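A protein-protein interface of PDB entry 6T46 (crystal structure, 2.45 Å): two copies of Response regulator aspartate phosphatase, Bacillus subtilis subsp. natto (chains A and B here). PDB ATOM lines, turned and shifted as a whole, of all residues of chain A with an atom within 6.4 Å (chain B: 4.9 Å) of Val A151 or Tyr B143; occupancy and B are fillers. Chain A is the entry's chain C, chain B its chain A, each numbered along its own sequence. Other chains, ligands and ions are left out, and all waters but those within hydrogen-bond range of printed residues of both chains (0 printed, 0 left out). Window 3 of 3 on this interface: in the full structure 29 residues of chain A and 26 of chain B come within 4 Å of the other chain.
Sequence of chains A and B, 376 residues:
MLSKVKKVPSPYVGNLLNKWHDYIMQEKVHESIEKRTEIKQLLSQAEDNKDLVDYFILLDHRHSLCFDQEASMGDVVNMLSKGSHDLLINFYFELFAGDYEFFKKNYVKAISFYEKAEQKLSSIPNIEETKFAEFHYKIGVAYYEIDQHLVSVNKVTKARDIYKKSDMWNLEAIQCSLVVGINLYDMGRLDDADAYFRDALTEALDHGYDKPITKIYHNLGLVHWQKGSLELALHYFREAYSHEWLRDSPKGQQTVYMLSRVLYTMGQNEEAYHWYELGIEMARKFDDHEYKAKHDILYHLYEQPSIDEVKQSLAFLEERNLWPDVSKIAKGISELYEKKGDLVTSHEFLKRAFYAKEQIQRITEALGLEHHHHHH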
ATOM      1  N   ILE A 139      -9.563  12.665   6.515  1.00  0.00           N
ATOM      2  CA  ILE A 139     -10.790  12.025   6.044  1.00  0.00           C
ATOM      3  C   ILE A 139     -10.505  10.613   5.550  1.00  0.00           C
ATOM      4  O   ILE A 139     -11.206   9.664   5.929  1.00  0.00           O
ATOM      5  CB  ILE A 139     -11.475  12.896   4.984  1.00  0.00           C
ATOM      6  CG1 ILE A 139     -11.805  14.246   5.624  1.00  0.00           C
ATOM      7  CG2 ILE A 139     -12.702  12.225   4.499  1.00  0.00           C
ATOM      8  CD1 ILE A 139     -12.391  15.255   4.663  1.00  0.00           C
ATOM      9  N   GLY A 140      -9.451  10.445   4.738  1.00  0.00           N
ATOM     10  CA  GLY A 140      -9.109   9.125   4.233  1.00  0.00           C
ATOM     11  C   GLY A 140      -8.843   8.117   5.337  1.00  0.00           C
ATOM     12  O   GLY A 140      -9.361   6.989   5.303  1.00  0.00           O
ATOM     13  N   TYR A 143     -12.236   7.158   6.798  1.00  0.00           N
ATOM     14  CA  TYR A 143     -12.978   6.189   5.988  1.00  0.00           C
ATOM     15  C   TYR A 143     -12.394   4.799   6.146  1.00  0.00           C
ATOM     16  O   TYR A 143     -13.125   3.809   6.322  1.00  0.00           O
ATOM     17  CB  TYR A 143     -12.931   6.564   4.510  1.00  0.00           C
ATOM     18  CG  TYR A 143     -13.962   7.578   4.084  1.00  0.00           C
ATOM     19  CD1 TYR A 143     -15.323   7.365   4.283  1.00  0.00           C
ATOM     20  CD2 TYR A 143     -13.571   8.731   3.443  1.00  0.00           C
ATOM     21  CE1 TYR A 143     -16.253   8.307   3.882  1.00  0.00           C
ATOM     22  CE2 TYR A 143     -14.482   9.654   3.034  1.00  0.00           C
ATOM     23  CZ  TYR A 143     -15.818   9.434   3.254  1.00  0.00           C
ATOM     24  OH  TYR A 143     -16.694  10.393   2.827  1.00  0.00           O
ATOM     25  N   GLN A 148     -14.350   1.850   4.406  1.00  0.00           N
ATOM     26  CA  GLN A 148     -14.754   2.412   3.127  1.00  0.00           C
ATOM     27  C   GLN A 148     -13.500   2.650   2.283  1.00  0.00           C
ATOM     28  O   GLN A 148     -13.072   3.787   2.057  1.00  0.00           O
ATOM     29  CB  GLN A 148     -15.508   3.699   3.375  1.00  0.00           C
ATOM     30  CG  GLN A 148     -16.766   3.438   4.155  1.00  0.00           C
ATOM     31  CD  GLN A 148     -17.950   3.206   3.283  1.00  0.00           C
ATOM     32  OE1 GLN A 148     -18.179   3.919   2.272  1.00  0.00           O
ATOM     33  NE2 GLN A 148     -18.711   2.198   3.638  1.00  0.00           N
ATOM     34  N   HIS A 149     -12.917   1.536   1.806  1.00  0.00           N
ATOM     35  CA  HIS A 149     -11.557   1.540   1.259  1.00  0.00           C
ATOM     36  C   HIS A 149     -11.457   2.310  -0.047  1.00  0.00           C
ATOM     37  O   HIS A 149     -10.465   3.022  -0.283  1.00  0.00           O
ATOM     38  CB  HIS A 149     -11.086   0.117   1.063  1.00  0.00           C
ATOM     39  CG  HIS A 149     -11.155  -0.688   2.316  1.00  0.00           C
ATOM     40  ND1 HIS A 149     -10.389  -0.397   3.420  1.00  0.00           N
ATOM     41  CD2 HIS A 149     -11.950  -1.726   2.673  1.00  0.00           C
ATOM     42  CE1 HIS A 149     -10.675  -1.246   4.394  1.00  0.00           C
ATOM     43  NE2 HIS A 149     -11.630  -2.059   3.972  1.00  0.00           N
ATOM     44  N   LEU A 150     -12.454   2.215  -0.916  1.00  0.00           N
ATOM     45  CA  LEU A 150     -12.300   2.905  -2.197  1.00  0.00           C
ATOM     46  C   LEU A 150     -12.122   4.393  -2.016  1.00  0.00           C
ATOM     47  O   LEU A 150     -11.202   4.978  -2.582  1.00  0.00           O
ATOM     48  CB  LEU A 150     -13.487   2.664  -3.094  1.00  0.00           C
ATOM     49  CG  LEU A 150     -13.150   1.506  -4.000  1.00  0.00           C
ATOM     50  CD1 LEU A 150     -12.161   2.009  -5.046  1.00  0.00           C
ATOM     51  CD2 LEU A 150     -12.598   0.364  -3.147  1.00  0.00           C
ATOM     52  N   VAL A 151     -13.009   5.030  -1.245  1.00  0.00           N
ATOM     53  CA  VAL A 151     -12.867   6.465  -0.992  1.00  0.00           C
ATOM     54  C   VAL A 151     -11.595   6.740  -0.208  1.00  0.00           C
ATOM     55  O   VAL A 151     -10.905   7.738  -0.450  1.00  0.00           O
ATOM     56  CB  VAL A 151     -14.096   7.012  -0.244  1.00  0.00           C
ATOM     57  CG1 VAL A 151     -14.222   8.493  -0.443  1.00  0.00           C
ATOM     58  CG2 VAL A 151     -15.337   6.302  -0.697  1.00  0.00           C
ATOM     59  N   SER A 152     -11.259   5.851   0.738  1.00  0.00           N
ATOM     60  CA  SER A 152     -10.085   6.070   1.569  1.00  0.00           C
ATOM     61  C   SER A 152      -8.865   6.237   0.692  1.00  0.00           C
ATOM     62  O   SER A 152      -8.119   7.214   0.816  1.00  0.00           O
ATOM     63  CB  SER A 152      -9.910   4.914   2.537  1.00  0.00           C
ATOM     64  OG  SER A 152      -8.869   5.208   3.456  1.00  0.00           O
ATOM     65  N   VAL A 153      -8.676   5.311  -0.244  1.00  0.00           N
ATOM     66  CA  VAL A 153      -7.594   5.439  -1.220  1.00  0.00           C
ATOM     67  C   VAL A 153      -7.731   6.709  -2.048  1.00  0.00           C
ATOM     68  O   VAL A 153      -6.730   7.283  -2.500  1.00  0.00           O
ATOM     69  CB  VAL A 153      -7.596   4.192  -2.113  1.00  0.00           C
ATOM     70  CG1 VAL A 153      -6.686   4.392  -3.290  1.00  0.00           C
ATOM     71  CG2 VAL A 153      -7.277   2.947  -1.269  1.00  0.00           C
ATOM     72  N   ASN A 154      -8.956   7.161  -2.310  1.00  0.00           N
ATOM     73  CA  ASN A 154      -9.116   8.382  -3.099  1.00  0.00           C
ATOM     74  C   ASN A 154      -8.573   9.593  -2.340  1.00  0.00           C
ATOM     75  O   ASN A 154      -7.713  10.328  -2.849  1.00  0.00           O
ATOM     76  CB  ASN A 154     -10.598   8.564  -3.445  1.00  0.00           C
ATOM     77  CG  ASN A 154     -10.879   9.769  -4.327  1.00  0.00           C
ATOM     78  OD1 ASN A 154     -10.696  10.926  -3.921  1.00  0.00           O
ATOM     79  ND2 ASN A 154     -11.386   9.503  -5.534  1.00  0.00           N
ATOM     80  N   LYS A 155      -9.046   9.805  -1.105  1.00  0.00           N
ATOM     81  CA  LYS A 155      -8.598  10.970  -0.335  1.00  0.00           C
ATOM     82  C   LYS A 155      -7.106  10.873  -0.018  1.00  0.00           C
ATOM     83  O   LYS A 155      -6.348  11.828  -0.227  1.00  0.00           O
ATOM     84  CB  LYS A 155      -9.438  11.124   0.937  1.00  0.00           C
ATOM     85  CG  LYS A 155     -10.963  11.257   0.690  1.00  0.00           C
ATOM     86  CD  LYS A 155     -11.357  12.597   0.122  1.00  0.00           C
ATOM     87  CE  LYS A 155     -11.661  13.611   1.230  1.00  0.00           C
ATOM     88  NZ  LYS A 155     -11.705  15.055   0.737  1.00  0.00           N
ATOM     89  N   VAL A 156      -6.649   9.712   0.457  1.00  0.00           N
ATOM     90  CA  VAL A 156      -5.250   9.617   0.854  1.00  0.00           C
ATOM     91  C   VAL A 156      -4.344   9.886  -0.331  1.00  0.00           C
ATOM     92  O   VAL A 156      -3.363  10.617  -0.191  1.00  0.00           O
ATOM     93  CB  VAL A 156      -4.941   8.253   1.474  1.00  0.00           C
ATOM     94  CG1 VAL A 156      -3.454   8.141   1.733  1.00  0.00           C
ATOM     95  CG2 VAL A 156      -5.668   8.105   2.745  1.00  0.00           C
ATOM     96  N   LYS A 158      -5.072  11.870  -2.788  1.00  0.00           N
ATOM     97  CA  LYS A 158      -5.088  13.328  -2.978  1.00  0.00           C
ATOM     98  C   LYS A 158      -4.066  13.998  -2.077  1.00  0.00           C
ATOM     99  O   LYS A 158      -3.309  14.868  -2.528  1.00  0.00           O
ATOM    100  CB  LYS A 158      -6.473  13.937  -2.728  1.00  0.00           C
ATOM    101  CG  LYS A 158      -7.320  13.969  -3.961  1.00  0.00           C
ATOM    102  CD  LYS A 158      -8.786  13.772  -3.706  1.00  0.00           C
ATOM    103  CE  LYS A 158      -9.563  13.757  -5.040  1.00  0.00           C
ATOM    104  NZ  LYS A 158     -11.000  13.324  -4.883  1.00  0.00           N
ATOM    105  N   ILE B 111     -15.845   8.414 -11.632  1.00  0.00           N
ATOM    106  CA  ILE B 111     -15.658   9.282 -10.477  1.00  0.00           C
ATOM    107  C   ILE B 111     -14.435  10.170 -10.668  1.00  0.00           C
ATOM    108  O   ILE B 111     -14.438  11.354 -10.307  1.00  0.00           O
ATOM    109  CB  ILE B 111     -15.541   8.441  -9.215  1.00  0.00           C
ATOM    110  CG1 ILE B 111     -16.876   7.771  -8.953  1.00  0.00           C
ATOM    111  CG2 ILE B 111     -15.183   9.331  -8.100  1.00  0.00           C
ATOM    112  CD1 ILE B 111     -16.870   6.911  -7.713  1.00  0.00           C
ATOM    113  N   GLU B 115     -14.977  14.151 -10.753  1.00  0.00           N
ATOM    114  CA  GLU B 115     -14.361  14.976  -9.728  1.00  0.00           C
ATOM    115  C   GLU B 115     -13.504  16.072 -10.335  1.00  0.00           C
ATOM    116  O   GLU B 115     -13.471  17.185  -9.798  1.00  0.00           O
ATOM    117  CB  GLU B 115     -13.575  14.129  -8.739  1.00  0.00           C
ATOM    118  CG  GLU B 115     -14.505  13.326  -7.844  1.00  0.00           C
ATOM    119  CD  GLU B 115     -13.783  12.688  -6.686  1.00  0.00           C
ATOM    120  OE1 GLU B 115     -14.481  12.284  -5.724  1.00  0.00           O
ATOM    121  OE2 GLU B 115     -12.539  12.518  -6.768  1.00  0.00           O
ATOM    122  N   ILE B 139     -21.661  11.521  -8.811  1.00  0.00           N
ATOM    123  CA  ILE B 139     -20.575  10.868  -8.083  1.00  0.00           C
ATOM    124  C   ILE B 139     -21.133   9.880  -7.069  1.00  0.00           C
ATOM    125  O   ILE B 139     -20.627   8.761  -6.923  1.00  0.00           O
ATOM    126  CB  ILE B 139     -19.658  11.920  -7.433  1.00  0.00           C
ATOM    127  CG1 ILE B 139     -19.112  12.837  -8.530  1.00  0.00           C
ATOM    128  CG2 ILE B 139     -18.536  11.244  -6.688  1.00  0.00           C
ATOM    129  CD1 ILE B 139     -18.252  13.992  -8.051  1.00  0.00           C
ATOM    130  N   GLY B 140     -22.171  10.279  -6.340  1.00  0.00           N
ATOM    131  CA  GLY B 140     -22.758   9.383  -5.356  1.00  0.00           C
ATOM    132  C   GLY B 140     -23.270   8.083  -5.947  1.00  0.00           C
ATOM    133  O   GLY B 140     -23.199   7.031  -5.299  1.00  0.00           O
ATOM    134  N   VAL B 141     -23.891   8.147  -7.135  1.00  0.00           N
ATOM    135  CA  VAL B 141     -24.400   6.917  -7.749  1.00  0.00           C
ATOM    136  C   VAL B 141     -23.253   6.021  -8.185  1.00  0.00           C
ATOM    137  O   VAL B 141     -23.323   4.797  -8.036  1.00  0.00           O
ATOM    138  CB  VAL B 141     -25.373   7.211  -8.904  1.00  0.00           C
ATOM    139  CG1 VAL B 141     -25.438   6.045  -9.838  1.00  0.00           C
ATOM    140  CG2 VAL B 141     -26.751   7.377  -8.342  1.00  0.00           C
ATOM    141  N   ALA B 142     -22.188   6.603  -8.739  1.00  0.00           N
ATOM    142  CA  ALA B 142     -21.044   5.774  -9.106  1.00  0.00           C
ATOM    143  C   ALA B 142     -20.415   5.139  -7.871  1.00  0.00           C
ATOM    144  O   ALA B 142     -20.165   3.927  -7.848  1.00  0.00           O
ATOM    145  CB  ALA B 142     -20.013   6.594  -9.871  1.00  0.00           C
ATOM    146  N   TYR B 143     -20.243   5.909  -6.794  1.00  0.00           N
ATOM    147  CA  TYR B 143     -19.767   5.299  -5.546  1.00  0.00           C
ATOM    148  C   TYR B 143     -20.719   4.224  -5.058  1.00  0.00           C
ATOM    149  O   TYR B 143     -20.286   3.219  -4.491  1.00  0.00           O
ATOM    150  CB  TYR B 143     -19.585   6.334  -4.442  1.00  0.00           C
ATOM    151  CG  TYR B 143     -18.232   6.972  -4.443  1.00  0.00           C
ATOM    152  CD1 TYR B 143     -17.079   6.193  -4.342  1.00  0.00           C
ATOM    153  CD2 TYR B 143     -18.090   8.341  -4.488  1.00  0.00           C
ATOM    154  CE1 TYR B 143     -15.813   6.773  -4.316  1.00  0.00           C
ATOM    155  CE2 TYR B 143     -16.836   8.927  -4.470  1.00  0.00           C
ATOM    156  CZ  TYR B 143     -15.700   8.133  -4.385  1.00  0.00           C
ATOM    157  OH  TYR B 143     -14.444   8.708  -4.361  1.00  0.00           O
ATOM    158  N   TYR B 144     -22.021   4.427  -5.226  1.00  0.00           N
ATOM    159  CA  TYR B 144     -22.954   3.375  -4.831  1.00  0.00           C
ATOM    160  C   TYR B 144     -22.759   2.108  -5.654  1.00  0.00           C
ATOM    161  O   TYR B 144     -22.880   0.992  -5.131  1.00  0.00           O
ATOM    162  CB  TYR B 144     -24.386   3.855  -4.980  1.00  0.00           C
ATOM    163  CG  TYR B 144     -25.360   2.722  -5.074  1.00  0.00           C
ATOM    164  CD1 TYR B 144     -25.771   2.050  -3.939  1.00  0.00           C
ATOM    165  CD2 TYR B 144     -25.865   2.316  -6.299  1.00  0.00           C
ATOM    166  CE1 TYR B 144     -26.680   1.014  -4.019  1.00  0.00           C
ATOM    167  CE2 TYR B 144     -26.778   1.280  -6.390  1.00  0.00           C
ATOM    168  CZ  TYR B 144     -27.181   0.625  -5.249  1.00  0.00           C
ATOM    169  OH  TYR B 144     -28.086  -0.423  -5.316  1.00  0.00           O
ATOM    170  N   GLU B 145     -22.505   2.253  -6.953  1.00  0.00           N
ATOM    171  CA  GLU B 145     -22.403   1.061  -7.779  1.00  0.00           C
ATOM    172  C   GLU B 145     -21.194   0.229  -7.421  1.00  0.00           C
ATOM    173  O   GLU B 145     -21.186  -0.971  -7.692  1.00  0.00           O
ATOM    174  CB  GLU B 145     -22.375   1.418  -9.256  1.00  0.00           C
ATOM    175  CG  GLU B 145     -23.713   1.893  -9.792  1.00  0.00           C
ATOM    176  CD  GLU B 145     -24.733   0.771  -9.823  1.00  0.00           C
ATOM    177  OE1 GLU B 145     -25.905   1.001 -10.214  1.00  0.00           O
ATOM    178  OE2 GLU B 145     -24.347  -0.368  -9.497  1.00  0.00           O
ATOM    179  N   ILE B 146     -20.151   0.834  -6.873  1.00  0.00           N
ATOM    180  CA  ILE B 146     -19.011   0.073  -6.394  1.00  0.00           C
ATOM    181  C   ILE B 146     -19.084  -0.110  -4.878  1.00  0.00           C
ATOM    182  O   ILE B 146     -18.058  -0.275  -4.221  1.00  0.00           O
ATOM    183  CB  ILE B 146     -17.666   0.676  -6.824  1.00  0.00           C
ATOM    184  CG1 ILE B 146     -17.604   2.177  -6.622  1.00  0.00           C
ATOM    185  CG2 ILE B 146     -17.455   0.444  -8.307  1.00  0.00           C
ATOM    186  CD1 ILE B 146     -16.230   2.712  -6.931  1.00  0.00           C
ATOM    187  N   ASP B 147     -20.272   0.031  -4.302  1.00  0.00           N
ATOM    188  CA  ASP B 147     -20.533  -0.399  -2.927  1.00  0.00           C
ATOM    189  C   ASP B 147     -19.783   0.432  -1.885  1.00  0.00           C
ATOM    190  O   ASP B 147     -19.345  -0.093  -0.865  1.00  0.00           O
ATOM    191  CB  ASP B 147     -20.212  -1.887  -2.777  1.00  0.00           C
ATOM    192  CG  ASP B 147     -21.215  -2.777  -3.535  1.00  0.00           C
ATOM    193  OD1 ASP B 147     -22.342  -3.018  -3.014  1.00  0.00           O
ATOM    194  OD2 ASP B 147     -20.872  -3.196  -4.679  1.00  0.00           O
ATOM    195  N   GLN B 148     -19.605   1.730  -2.150  1.00  0.00           N
ATOM    196  CA  GLN B 148     -19.098   2.676  -1.159  1.00  0.00           C
ATOM    197  C   GLN B 148     -20.290   3.428  -0.569  1.00  0.00           C
ATOM    198  O   GLN B 148     -20.619   4.542  -0.980  1.00  0.00           O
ATOM    199  CB  GLN B 148     -18.100   3.625  -1.791  1.00  0.00           C
ATOM    200  CG  GLN B 148     -16.875   2.892  -2.306  1.00  0.00           C
ATOM    201  CD  GLN B 148     -15.974   2.325  -1.233  1.00  0.00           C
ATOM    202  OE1 GLN B 148     -15.751   1.116  -1.209  1.00  0.00           O
ATOM    203  NE2 GLN B 148     -15.372   3.192  -0.405  1.00  0.00           N
ATOM    204  N   VAL B 151     -20.102   7.152   1.701  1.00  0.00           N
ATOM    205  CA  VAL B 151     -19.871   8.341   0.873  1.00  0.00           C
ATOM    206  C   VAL B 151     -21.024   8.536  -0.100  1.00  0.00           C
ATOM    207  O   VAL B 151     -21.375   9.672  -0.433  1.00  0.00           O
ATOM    208  CB  VAL B 151     -18.517   8.288   0.141  1.00  0.00           C
ATOM    209  CG1 VAL B 151     -18.606   7.443  -1.112  1.00  0.00           C
ATOM    210  CG2 VAL B 151     -18.127   9.682  -0.247  1.00  0.00           C
ATOM    211  N   SER B 152     -21.616   7.446  -0.595  1.00  0.00           N
ATOM    212  CA  SER B 152     -22.751   7.597  -1.498  1.00  0.00           C
ATOM    213  C   SER B 152     -23.912   8.299  -0.803  1.00  0.00           C
ATOM    214  O   SER B 152     -24.440   9.301  -1.305  1.00  0.00           O
ATOM    215  CB  SER B 152     -23.210   6.253  -2.027  1.00  0.00           C
ATOM    216  OG  SER B 152     -24.187   6.490  -3.020  1.00  0.00           O
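The side-chain carboxylate of Glu B115 is in hydrogen-bond range of the side-chain amide nitrogen of Asn A154 (3.5 Å).
OE2 of Glu B115 lies within salt-bridge range of NZ of Lys A158.
ND2 of Asn A154 sits at hydrogen-bond distance from OH of Tyr B143, at 3.4 Å.
NE2 of Gln B148 sits close to O of Gln A148, 3.4 Å away.
NE2 of Gln B148 lies close to N of Leu A150 (3.1 Å).
N of Val A151 lies close to NE2 of Gln B148, at 3.1 Å.
The backbone NH (N) of Gln B148 sits at hydrogen-bond distance from the backbone carbonyl oxygen (O) of Tyr B143 (2.9 Å).
The backbone NH (N) of Gln A148 sits at hydrogen-bond distance from the backbone carbonyl oxygen (O) of Tyr A143, 3.0 Å away.
The side-chain amide oxygen (OD1) of Asn A154 lies within hydrogen-bond range of the side-chain amino group (NZ) of Lys A158 (2.6 Å).
CG2 of Val B151 touches OH of Tyr A143, 3.5 Å away.
Gln A148 touches Val B151.
Gln B148 touches His A149 (NE2 to N, 3.7 Å).
Tyr B143 touches Val A151 (CE1 to CG2, 3.7 Å).
Val B151 touches Val A151.
Printed residues of chain B within 4 Å of Gln A148: Gln B148 (3.3 Å) and Val B151 (3.8 Å).
Val A151 touches just these residues of chain B: Tyr B143, Gln B148 and Val B151.
Printed residues of chain B within 4 Å of Lys A158: Glu B115.
Gly B140 touches none of the printed residues of chain A.
Ile B146 touches none of the printed residues of chain A.
The nearest printed residue of chain B that does not touch Val A151 is Ser B152 (6.4 Å).
The nearest residue of chain A that does not touch Tyr B143 is Leu A150 (4.9 Å).
Hydrophobic or aromatic side chains of chain B that line the printed part of chain A: Tyr B143 and Val B151.
Hydrophobic or aromatic side chains of chain A within 4 Å of the printed part of chain B: Tyr A143, Leu A150 and Val A151.
Among the printed residues, Asp or Glu carboxylates within 4 Å of a Lys or Arg side-chain nitrogen of the other chain: Lys A158 with Glu B115 (2.6 Å).
Tyr A143 touches Val B151, and with the chains exchanged Val A151 touches Tyr B143.
Gln A148 touches its own counterpart, Gln B148.
Gln A148 touches Val B151, and with the chains exchanged Val A151 touches Gln B148.
Val B151 touches its own counterpart, Val A151.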
